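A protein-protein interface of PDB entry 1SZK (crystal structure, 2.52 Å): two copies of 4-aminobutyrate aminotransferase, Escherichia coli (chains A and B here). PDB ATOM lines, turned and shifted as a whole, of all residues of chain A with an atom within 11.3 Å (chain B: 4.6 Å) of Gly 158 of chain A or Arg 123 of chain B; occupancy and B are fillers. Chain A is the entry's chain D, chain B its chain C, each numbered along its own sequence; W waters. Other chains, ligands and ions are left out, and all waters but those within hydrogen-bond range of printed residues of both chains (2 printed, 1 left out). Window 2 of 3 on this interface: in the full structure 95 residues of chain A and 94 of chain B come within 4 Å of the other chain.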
ATOM      1  N   ARG A  17       3.032   8.710  22.978  1.00  0.00           N
ATOM      2  CA  ARG A  17       3.333   9.377  21.717  1.00  0.00           C
ATOM      3  C   ARG A  17       4.372   8.602  20.905  1.00  0.00           C
ATOM      4  O   ARG A  17       4.565   8.853  19.707  1.00  0.00           O
ATOM      5  CB  ARG A  17       3.818  10.811  21.973  1.00  0.00           C
ATOM      6  CG  ARG A  17       4.832  10.944  23.088  1.00  0.00           C
ATOM      7  CD  ARG A  17       5.708  12.179  22.893  1.00  0.00           C
ATOM      8  NE  ARG A  17       6.896  12.089  23.732  1.00  0.00           N
ATOM      9  CZ  ARG A  17       8.090  12.570  23.402  1.00  0.00           C
ATOM     10  NH1 ARG A  17       8.264  13.188  22.238  1.00  0.00           N
ATOM     11  NH2 ARG A  17       9.115  12.416  24.233  1.00  0.00           N
ATOM     12  N   ARG A 141      11.734  -4.303  15.475  1.00  0.00           N
ATOM     13  CA  ARG A 141      11.902  -3.401  16.600  1.00  0.00           C
ATOM     14  C   ARG A 141      12.284  -3.993  17.941  1.00  0.00           C
ATOM     15  O   ARG A 141      12.013  -3.398  18.967  1.00  0.00           O
ATOM     16  CB  ARG A 141      10.646  -2.548  16.760  1.00  0.00           C
ATOM     17  CG  ARG A 141      10.285  -1.805  15.486  1.00  0.00           C
ATOM     18  CD  ARG A 141       9.686  -0.463  15.799  1.00  0.00           C
ATOM     19  NE  ARG A 141       9.109   0.176  14.622  1.00  0.00           N
ATOM     20  CZ  ARG A 141       8.821   1.469  14.563  1.00  0.00           C
ATOM     21  NH1 ARG A 141       9.065   2.250  15.611  1.00  0.00           N
ATOM     22  NH2 ARG A 141       8.282   1.978  13.467  1.00  0.00           N
ATOM     23  N   THR A 142      12.885  -5.173  17.945  1.00  0.00           N
ATOM     24  CA  THR A 142      13.344  -5.766  19.195  1.00  0.00           C
ATOM     25  C   THR A 142      14.762  -5.214  19.319  1.00  0.00           C
ATOM     26  O   THR A 142      15.306  -4.692  18.338  1.00  0.00           O
ATOM     27  CB  THR A 142      13.385  -7.321  19.118  1.00  0.00           C
ATOM     28  OG1 THR A 142      14.093  -7.729  17.940  1.00  0.00           O
ATOM     29  CG2 THR A 142      11.985  -7.891  19.064  1.00  0.00           C
ATOM     30  N   HIS A 143      15.367  -5.300  20.495  1.00  0.00           N
ATOM     31  CA  HIS A 143      16.719  -4.778  20.625  1.00  0.00           C
ATOM     32  C   HIS A 143      17.626  -5.251  19.506  1.00  0.00           C
ATOM     33  O   HIS A 143      18.246  -4.440  18.795  1.00  0.00           O
ATOM     34  CB  HIS A 143      17.346  -5.181  21.952  1.00  0.00           C
ATOM     35  CG  HIS A 143      16.889  -4.354  23.109  1.00  0.00           C
ATOM     36  ND1 HIS A 143      15.615  -4.442  23.628  1.00  0.00           N
ATOM     37  CD2 HIS A 143      17.545  -3.445  23.868  1.00  0.00           C
ATOM     38  CE1 HIS A 143      15.510  -3.626  24.662  1.00  0.00           C
ATOM     39  NE2 HIS A 143      16.668  -3.010  24.830  1.00  0.00           N
ATOM     40  N   TYR A 144      17.694  -6.566  19.327  1.00  0.00           N
ATOM     41  CA  TYR A 144      18.571  -7.093  18.305  1.00  0.00           C
ATOM     42  C   TYR A 144      18.167  -6.680  16.898  1.00  0.00           C
ATOM     43  O   TYR A 144      19.023  -6.283  16.111  1.00  0.00           O
ATOM     44  CB  TYR A 144      18.698  -8.613  18.407  1.00  0.00           C
ATOM     45  CG  TYR A 144      19.889  -9.120  17.635  1.00  0.00           C
ATOM     46  CD1 TYR A 144      21.145  -9.232  18.234  1.00  0.00           C
ATOM     47  CD2 TYR A 144      19.772  -9.441  16.285  1.00  0.00           C
ATOM     48  CE1 TYR A 144      22.248  -9.654  17.502  1.00  0.00           C
ATOM     49  CE2 TYR A 144      20.863  -9.858  15.541  1.00  0.00           C
ATOM     50  CZ  TYR A 144      22.093  -9.962  16.145  1.00  0.00           C
ATOM     51  OH  TYR A 144      23.175 -10.333  15.379  1.00  0.00           O
ATOM     52  N   THR A 145      16.881  -6.742  16.563  1.00  0.00           N
ATOM     53  CA  THR A 145      16.519  -6.326  15.213  1.00  0.00           C
ATOM     54  C   THR A 145      16.677  -4.822  14.992  1.00  0.00           C
ATOM     55  O   THR A 145      16.773  -4.373  13.842  1.00  0.00           O
ATOM     56  CB  THR A 145      15.097  -6.819  14.782  1.00  0.00           C
ATOM     57  OG1 THR A 145      14.118  -6.515  15.784  1.00  0.00           O
ATOM     58  CG2 THR A 145      15.138  -8.326  14.538  1.00  0.00           C
ATOM     59  N   LEU A 146      16.720  -4.039  16.076  1.00  0.00           N
ATOM     60  CA  LEU A 146      16.935  -2.602  15.930  1.00  0.00           C
ATOM     61  C   LEU A 146      18.409  -2.422  15.538  1.00  0.00           C
ATOM     62  O   LEU A 146      18.747  -1.548  14.738  1.00  0.00           O
ATOM     63  CB  LEU A 146      16.621  -1.850  17.229  1.00  0.00           C
ATOM     64  CG  LEU A 146      15.140  -1.604  17.570  1.00  0.00           C
ATOM     65  CD1 LEU A 146      15.034  -1.035  18.961  1.00  0.00           C
ATOM     66  CD2 LEU A 146      14.501  -0.662  16.567  1.00  0.00           C
ATOM     67  N   ALA A 147      19.283  -3.262  16.090  1.00  0.00           N
ATOM     68  CA  ALA A 147      20.712  -3.206  15.745  1.00  0.00           C
ATOM     69  C   ALA A 147      20.921  -3.602  14.282  1.00  0.00           C
ATOM     70  O   ALA A 147      21.809  -3.067  13.623  1.00  0.00           O
ATOM     71  CB  ALA A 147      21.510  -4.124  16.638  1.00  0.00           C
ATOM     72  N   LYS A 151      18.987   2.270  10.708  1.00  0.00           N
ATOM     73  CA  LYS A 151      18.358   3.560  10.977  1.00  0.00           C
ATOM     74  C   LYS A 151      18.179   3.679  12.480  1.00  0.00           C
ATOM     75  O   LYS A 151      17.483   2.867  13.083  1.00  0.00           O
ATOM     76  CB  LYS A 151      16.988   3.642  10.300  1.00  0.00           C
ATOM     77  CG  LYS A 151      16.216   4.924  10.612  1.00  0.00           C
ATOM     78  CD  LYS A 151      14.998   5.064   9.700  1.00  0.00           C
ATOM     79  CE  LYS A 151      14.382   6.465   9.758  1.00  0.00           C
ATOM     80  NZ  LYS A 151      13.318   6.641   8.719  1.00  0.00           N
ATOM     81  N   VAL A 152      18.797   4.681  13.091  1.00  0.00           N
ATOM     82  CA  VAL A 152      18.682   4.845  14.533  1.00  0.00           C
ATOM     83  C   VAL A 152      17.493   5.688  14.978  1.00  0.00           C
ATOM     84  O   VAL A 152      16.895   5.418  16.023  1.00  0.00           O
ATOM     85  CB  VAL A 152      19.945   5.498  15.137  1.00  0.00           C
ATOM     86  CG1 VAL A 152      19.885   5.414  16.667  1.00  0.00           C
ATOM     87  CG2 VAL A 152      21.195   4.830  14.584  1.00  0.00           C
ATOM     88  N   ASN A 153      17.161   6.711  14.191  1.00  0.00           N
ATOM     89  CA  ASN A 153      16.071   7.621  14.535  1.00  0.00           C
ATOM     90  C   ASN A 153      14.788   7.342  13.770  1.00  0.00           C
ATOM     91  O   ASN A 153      14.793   7.262  12.537  1.00  0.00           O
ATOM     92  CB  ASN A 153      16.516   9.062  14.285  1.00  0.00           C
ATOM     93  CG  ASN A 153      15.507  10.084  14.786  1.00  0.00           C
ATOM     94  OD1 ASN A 153      15.172  10.111  15.971  1.00  0.00           O
ATOM     95  ND2 ASN A 153      15.022  10.934  13.883  1.00  0.00           N
ATOM     96  N   PRO A 154      13.657   7.229  14.492  1.00  0.00           N
ATOM     97  CA  PRO A 154      13.536   7.347  15.952  1.00  0.00           C
ATOM     98  C   PRO A 154      13.567   6.000  16.663  1.00  0.00           C
ATOM     99  O   PRO A 154      13.574   5.944  17.899  1.00  0.00           O
ATOM    100  CB  PRO A 154      12.180   7.997  16.116  1.00  0.00           C
ATOM    101  CG  PRO A 154      11.375   7.207  15.095  1.00  0.00           C
ATOM    102  CD  PRO A 154      12.320   7.124  13.875  1.00  0.00           C
ATOM    103  N   TYR A 155      13.572   4.925  15.875  1.00  0.00           N
ATOM    104  CA  TYR A 155      13.570   3.560  16.400  1.00  0.00           C
ATOM    105  C   TYR A 155      14.423   3.308  17.650  1.00  0.00           C
ATOM    106  O   TYR A 155      14.058   2.460  18.447  1.00  0.00           O
ATOM    107  CB  TYR A 155      14.006   2.571  15.319  1.00  0.00           C
ATOM    108  CG  TYR A 155      13.294   2.690  13.988  1.00  0.00           C
ATOM    109  CD1 TYR A 155      13.991   2.475  12.807  1.00  0.00           C
ATOM    110  CD2 TYR A 155      11.937   3.015  13.901  1.00  0.00           C
ATOM    111  CE1 TYR A 155      13.371   2.586  11.573  1.00  0.00           C
ATOM    112  CE2 TYR A 155      11.298   3.122  12.656  1.00  0.00           C
ATOM    113  CZ  TYR A 155      12.033   2.905  11.501  1.00  0.00           C
ATOM    114  OH  TYR A 155      11.462   2.991  10.253  1.00  0.00           O
ATOM    115  N   SER A 156      15.536   4.025  17.833  1.00  0.00           N
ATOM    116  CA  SER A 156      16.406   3.806  19.007  1.00  0.00           C
ATOM    117  C   SER A 156      16.625   5.044  19.876  1.00  0.00           C
ATOM    118  O   SER A 156      17.190   4.958  20.971  1.00  0.00           O
ATOM    119  CB  SER A 156      17.793   3.293  18.570  1.00  0.00           C
ATOM    120  OG  SER A 156      17.707   2.201  17.665  1.00  0.00           O
ATOM    121  N   ALA A 157      16.178   6.191  19.379  1.00  0.00           N
ATOM    122  CA  ALA A 157      16.341   7.470  20.061  1.00  0.00           C
ATOM    123  C   ALA A 157      16.195   7.467  21.577  1.00  0.00           C
ATOM    124  O   ALA A 157      15.186   7.019  22.119  1.00  0.00           O
ATOM    125  CB  ALA A 157      15.387   8.475  19.465  1.00  0.00           C
ATOM    126  N   GLY A 158      17.219   7.973  22.252  1.00  0.00           N
ATOM    127  CA  GLY A 158      17.189   8.075  23.697  1.00  0.00           C
ATOM    128  C   GLY A 158      17.324   6.790  24.474  1.00  0.00           C
ATOM    129  O   GLY A 158      17.418   6.806  25.710  1.00  0.00           O
ATOM    130  N   MET A 159      17.361   5.668  23.762  1.00  0.00           N
ATOM    131  CA  MET A 159      17.462   4.371  24.422  1.00  0.00           C
ATOM    132  C   MET A 159      18.897   3.950  24.704  1.00  0.00           C
ATOM    133  O   MET A 159      19.149   3.122  25.579  1.00  0.00           O
ATOM    134  CB  MET A 159      16.753   3.321  23.579  1.00  0.00           C
ATOM    135  CG  MET A 159      15.267   3.547  23.452  1.00  0.00           C
ATOM    136  SD  MET A 159      14.569   2.398  22.286  1.00  0.00           S
ATOM    137  CE  MET A 159      13.665   3.432  21.068  1.00  0.00           C
ATOM    138  N   GLY A 160      19.841   4.542  23.983  1.00  0.00           N
ATOM    139  CA  GLY A 160      21.228   4.190  24.187  1.00  0.00           C
ATOM    140  C   GLY A 160      21.633   3.262  23.066  1.00  0.00           C
ATOM    141  O   GLY A 160      20.859   3.041  22.137  1.00  0.00           O
ATOM    142  N   LEU A 161      22.835   2.708  23.148  1.00  0.00           N
ATOM    143  CA  LEU A 161      23.319   1.817  22.104  1.00  0.00           C
ATOM    144  C   LEU A 161      22.663   0.444  22.103  1.00  0.00           C
ATOM    145  O   LEU A 161      22.553  -0.216  23.136  1.00  0.00           O
ATOM    146  CB  LEU A 161      24.833   1.669  22.213  1.00  0.00           C
ATOM    147  CG  LEU A 161      25.576   2.976  21.929  1.00  0.00           C
ATOM    148  CD1 LEU A 161      27.039   2.812  22.300  1.00  0.00           C
ATOM    149  CD2 LEU A 161      25.416   3.368  20.469  1.00  0.00           C
ATOM    150  N   MET A 162      22.213   0.031  20.924  1.00  0.00           N
ATOM    151  CA  MET A 162      21.592  -1.274  20.742  1.00  0.00           C
ATOM    152  C   MET A 162      22.679  -2.362  20.782  1.00  0.00           C
ATOM    153  O   MET A 162      23.856  -2.049  20.737  1.00  0.00           O
ATOM    154  CB  MET A 162      20.847  -1.292  19.408  1.00  0.00           C
ATOM    155  CG  MET A 162      19.528  -0.524  19.437  1.00  0.00           C
ATOM    156  SD  MET A 162      18.484  -1.179  20.764  1.00  0.00           S
ATOM    157  CE  MET A 162      18.786   0.011  22.042  1.00  0.00           C
ATOM    158  N   PRO A 163      22.294  -3.650  20.877  1.00  0.00           N
ATOM    159  CA  PRO A 163      23.257  -4.762  20.923  1.00  0.00           C
ATOM    160  C   PRO A 163      24.448  -4.637  19.959  1.00  0.00           C
ATOM    161  O   PRO A 163      24.341  -4.056  18.867  1.00  0.00           O
ATOM    162  CB  PRO A 163      22.392  -5.967  20.612  1.00  0.00           C
ATOM    163  CG  PRO A 163      21.106  -5.613  21.300  1.00  0.00           C
ATOM    164  CD  PRO A 163      20.911  -4.168  20.880  1.00  0.00           C
ATOM    165  N   GLY A 164      25.587  -5.176  20.377  1.00  0.00           N
ATOM    166  CA  GLY A 164      26.778  -5.102  19.553  1.00  0.00           C
ATOM    167  C   GLY A 164      26.970  -6.312  18.655  1.00  0.00           C
ATOM    168  O   GLY A 164      26.114  -7.191  18.580  1.00  0.00           O
ATOM    169  N   VAL B 119      11.362  -2.548  28.200  1.00  0.00           N
ATOM    170  CA  VAL B 119      12.754  -2.244  28.498  1.00  0.00           C
ATOM    171  C   VAL B 119      13.187  -1.028  27.691  1.00  0.00           C
ATOM    172  O   VAL B 119      13.872  -0.141  28.211  1.00  0.00           O
ATOM    173  CB  VAL B 119      13.675  -3.456  28.211  1.00  0.00           C
ATOM    174  CG1 VAL B 119      15.134  -3.033  28.296  1.00  0.00           C
ATOM    175  CG2 VAL B 119      13.400  -4.567  29.239  1.00  0.00           C
ATOM    176  N   LYS B 120      12.774  -0.979  26.431  1.00  0.00           N
ATOM    177  CA  LYS B 120      13.099   0.160  25.592  1.00  0.00           C
ATOM    178  C   LYS B 120      12.540   1.406  26.282  1.00  0.00           C
ATOM    179  O   LYS B 120      13.235   2.416  26.444  1.00  0.00           O
ATOM    180  CB  LYS B 120      12.463   0.006  24.212  1.00  0.00           C
ATOM    181  CG  LYS B 120      12.996  -1.159  23.412  1.00  0.00           C
ATOM    182  CD  LYS B 120      12.652  -1.041  21.935  1.00  0.00           C
ATOM    183  CE  LYS B 120      11.167  -1.049  21.694  1.00  0.00           C
ATOM    184  NZ  LYS B 120      10.884  -1.054  20.236  1.00  0.00           N
ATOM    185  N   ILE B 121      11.282   1.314  26.704  1.00  0.00           N
ATOM    186  CA  ILE B 121      10.609   2.412  27.384  1.00  0.00           C
ATOM    187  C   ILE B 121      11.386   2.843  28.636  1.00  0.00           C
ATOM    188  O   ILE B 121      11.716   4.023  28.800  1.00  0.00           O
ATOM    189  CB  ILE B 121       9.154   2.004  27.756  1.00  0.00           C
ATOM    190  CG1 ILE B 121       8.319   1.896  26.472  1.00  0.00           C
ATOM    191  CG2 ILE B 121       8.548   3.011  28.760  1.00  0.00           C
ATOM    192  CD1 ILE B 121       6.928   1.345  26.666  1.00  0.00           C
ATOM    193  N   ALA B 122      11.687   1.887  29.506  1.00  0.00           N
ATOM    194  CA  ALA B 122      12.431   2.195  30.722  1.00  0.00           C
ATOM    195  C   ALA B 122      13.757   2.888  30.410  1.00  0.00           C
ATOM    196  O   ALA B 122      14.138   3.834  31.095  1.00  0.00           O
ATOM    197  CB  ALA B 122      12.685   0.922  31.529  1.00  0.00           C
ATOM    198  N   ARG B 123      14.453   2.419  29.375  1.00  0.00           N
ATOM    199  CA  ARG B 123      15.741   2.995  28.991  1.00  0.00           C
ATOM    200  C   ARG B 123      15.625   4.448  28.547  1.00  0.00           C
ATOM    201  O   ARG B 123      16.382   5.311  28.985  1.00  0.00           O
ATOM    202  CB  ARG B 123      16.388   2.154  27.878  1.00  0.00           C
ATOM    203  CG  ARG B 123      16.854   0.786  28.359  1.00  0.00           C
ATOM    204  CD  ARG B 123      17.428  -0.093  27.247  1.00  0.00           C
ATOM    205  NE  ARG B 123      18.560   0.537  26.575  1.00  0.00           N
ATOM    206  CZ  ARG B 123      19.499  -0.122  25.901  1.00  0.00           C
ATOM    207  NH1 ARG B 123      19.450  -1.445  25.807  1.00  0.00           N
ATOM    208  NH2 ARG B 123      20.493   0.547  25.328  1.00  0.00           N
ATOM    209  N   ALA B 124      14.673   4.715  27.671  1.00  0.00           N
ATOM    210  CA  ALA B 124      14.470   6.065  27.180  1.00  0.00           C
ATOM    211  C   ALA B 124      14.100   7.010  28.339  1.00  0.00           C
ATOM    212  O   ALA B 124      14.563   8.145  28.404  1.00  0.00           O
ATOM    213  CB  ALA B 124      13.373   6.064  26.112  1.00  0.00           C
ATOM    214  N   ALA B 125      13.281   6.522  29.260  1.00  0.00           N
ATOM    215  CA  ALA B 125      12.838   7.313  30.399  1.00  0.00           C
ATOM    216  C   ALA B 125      13.925   7.674  31.390  1.00  0.00           C
ATOM    217  O   ALA B 125      13.905   8.759  31.966  1.00  0.00           O
ATOM    218  CB  ALA B 125      11.735   6.580  31.123  1.00  0.00           C
ATOM    219  N   THR B 126      14.867   6.768  31.600  1.00  0.00           N
ATOM    220  CA  THR B 126      15.926   6.999  32.565  1.00  0.00           C
ATOM    221  C   THR B 126      17.245   7.364  31.918  1.00  0.00           C
ATOM    222  O   THR B 126      18.159   7.852  32.591  1.00  0.00           O
ATOM    223  CB  THR B 126      16.179   5.748  33.423  1.00  0.00           C
ATOM    224  OG1 THR B 126      16.850   4.763  32.629  1.00  0.00           O
ATOM    225  CG2 THR B 126      14.868   5.166  33.929  1.00  0.00           C
ATOM    226  N   LYS B 127      17.352   7.119  30.620  1.00  0.00           N
ATOM    227  CA  LYS B 127      18.588   7.406  29.904  1.00  0.00           C
ATOM    228  C   LYS B 127      19.681   6.446  30.383  1.00  0.00           C
ATOM    229  O   LYS B 127      20.831   6.841  30.559  1.00  0.00           O
ATOM    230  CB  LYS B 127      19.044   8.854  30.151  1.00  0.00           C
ATOM    231  CG  LYS B 127      18.074   9.938  29.693  1.00  0.00           C
ATOM    232  CD  LYS B 127      17.953   9.981  28.184  1.00  0.00           C
ATOM    233  CE  LYS B 127      17.191  11.222  27.721  1.00  0.00           C
ATOM    234  NZ  LYS B 127      17.938  12.490  27.982  1.00  0.00           N
ATOM    235  N   ARG B 128      19.312   5.187  30.595  1.00  0.00           N
ATOM    236  CA  ARG B 128      20.264   4.170  31.036  1.00  0.00           C
ATOM    237  C   ARG B 128      20.179   2.927  30.152  1.00  0.00           C
ATOM    238  O   ARG B 128      19.159   2.690  29.504  1.00  0.00           O
ATOM    239  CB  ARG B 128      19.982   3.787  32.478  1.00  0.00           C
ATOM    240  CG  ARG B 128      20.016   4.953  33.422  1.00  0.00           C
ATOM    241  CD  ARG B 128      19.582   4.509  34.790  1.00  0.00           C
ATOM    242  NE  ARG B 128      19.545   5.639  35.692  1.00  0.00           N
ATOM    243  CZ  ARG B 128      19.079   5.593  36.933  1.00  0.00           C
ATOM    244  NH1 ARG B 128      18.601   4.455  37.432  1.00  0.00           N
ATOM    245  NH2 ARG B 128      19.088   6.697  37.670  1.00  0.00           N
ATOM    246  N   SER B 129      21.234   2.120  30.148  1.00  0.00           N
ATOM    247  CA  SER B 129      21.259   0.920  29.313  1.00  0.00           C
ATOM    248  C   SER B 129      21.149  -0.445  30.002  1.00  0.00           C
ATOM    249  O   SER B 129      20.748  -1.411  29.367  1.00  0.00           O
ATOM    250  CB  SER B 129      22.521   0.924  28.461  1.00  0.00           C
ATOM    251  OG  SER B 129      22.514   2.030  27.586  1.00  0.00           O
ATOM    252  N   ALA B 201      18.584   0.829  34.026  1.00  0.00           N
ATOM    253  CA  ALA B 201      17.320   1.385  33.575  1.00  0.00           C
ATOM    254  C   ALA B 201      16.154   0.787  34.340  1.00  0.00           C
ATOM    255  O   ALA B 201      15.231   1.504  34.725  1.00  0.00           O
ATOM    256  CB  ALA B 201      17.137   1.129  32.088  1.00  0.00           C
HETATM  257  O   HOH W   1      21.388  -2.696  23.767  1.00  0.00           O
HETATM  258  O   HOH W   2      24.620   2.747  25.660  1.00  0.00           O
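The backbone carbonyl oxygen (O) of Arg 141 of chain A sits at hydrogen-bond distance from the side-chain amino group (NZ) of Lys 120 of chain B, at 2.9 Å.
The guanidinium group (NH1) of Arg 123 of chain B sits at hydrogen-bond distance from a ring nitrogen (NE2) of His 143 of chain A, at 3.3 Å.
O of Met 159 of chain A sits at hydrogen-bond distance from NE of Arg 123 of chain B (2.8 Å).
NH2 of Arg 123 of chain B lies within hydrogen-bond range of O of Leu 161 of chain A (3.1 Å).
Val 119 of chain B touches His 143 of chain A.
CG of Lys 120 of chain B touches CE1 of His 143 of chain A (3.7 Å).
Leu 146 of chain A touches Lys 120 of chain B.
O of Gly 158 of chain A touches O of Arg 123 of chain B, at 3.7 Å.
Gly 158 of chain A touches Ala 124 of chain B.
Met 159 of chain A touches Lys 120 of chain B.
Arg 128 of chain B touches Met 159 of chain A (O to O, 3.9 Å).
Gly 160 of chain A touches Arg 123 of chain B.
Arg 123 of chain B touches Met 162 of chain A (NH2 to CE, 3.7 Å).
The backbone carbonyl oxygen (O) of Arg 123 of chain B lies within hydrogen-bond range of the backbone NH (N) of Arg 128 of chain B.
The guanidinium group (NH2) of Arg 123 of chain B lies within hydrogen-bond range of the side-chain hydroxyl (OG) of Ser 129 of chain B (3.4 Å).
The backbone NH of Arg 128 of chain B sits at hydrogen-bond distance from the side-chain hydroxyl of Thr 126 of chain B (3.2 Å).
The backbone NH of Arg 141 of chain A lies within hydrogen-bond range of the side-chain hydroxyl of Thr 145 of chain A, 3.3 Å away.
No position is printed for both chains.
Of the 13 pairs that touch across the chains among the printed residues, none has its exchanged pair printed and touching as well.
Of the 22 printed residues of chain A, 8 touch a printed residue of chain B.
Along chain A the printed residues that touch a printed residue of chain B span positions 141 to 162.
Of the 12 printed residues of chain B, 5 touch a printed residue of chain A.
Hydrophobic or aromatic side chains of chain B within 4 Å of the printed part of chain A: Val 119.
Arg 123 of chain B touches six residues of chain A.
Val 119 of chain B touches just one residue of chain A: His 143.
Ala 122 of chain B touches none of the printed residues of chain A.
Ala 124 of chain B touches just one residue of chain A: Gly 158 (3.4 Å).
No residue of chain A comes within 4 Å of Ala 125 of chain B.
No residue of chain A comes within 4 Å of Thr 126 of chain B.
No residue of chain A comes within 4 Å of Lys 127 of chain B.
No residue of chain A comes within 4 Å of Ser 129 of chain B.
No residue of chain A comes within 4 Å of Ala 201 of chain B.
Of the printed residues of chain B, Leu 161 of chain A touches Arg 123 (3.1 Å).
Printed residues of chain B within 4 Å of Gly 160 of chain A: Arg 123 (3.7 Å).
Of the printed residues of chain B, Arg 141 of chain A touches Lys 120.
Thr 142 of chain A touches none of the printed residues of chain B.
Ile 121 of chain B touches none of the printed residues of chain A.
The nearest residue of chain B that does not touch Gly 158 of chain A is Lys 127 of chain B (4.1 Å).
The nearest residue of chain A that does not touch Arg 123 of chain B is Pro 163 of chain A (5.8 Å).
The nearest printed residue of chain A that does not touch Lys 120 of chain B is Tyr 155 of chain A (5.1 Å).
Water W1 lies within hydrogen-bond range of the backbone carbonyl oxygen of Leu 161 of chain A (2.8 Å) and the guanidinium group of Arg 123 of chain B (3.1 Å).
Water W2 lies within hydrogen-bond range of the side-chain hydroxyl of Ser 129 of chain B (2.9 Å) and the backbone NH of Leu 161 of chain A (3.1 Å).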
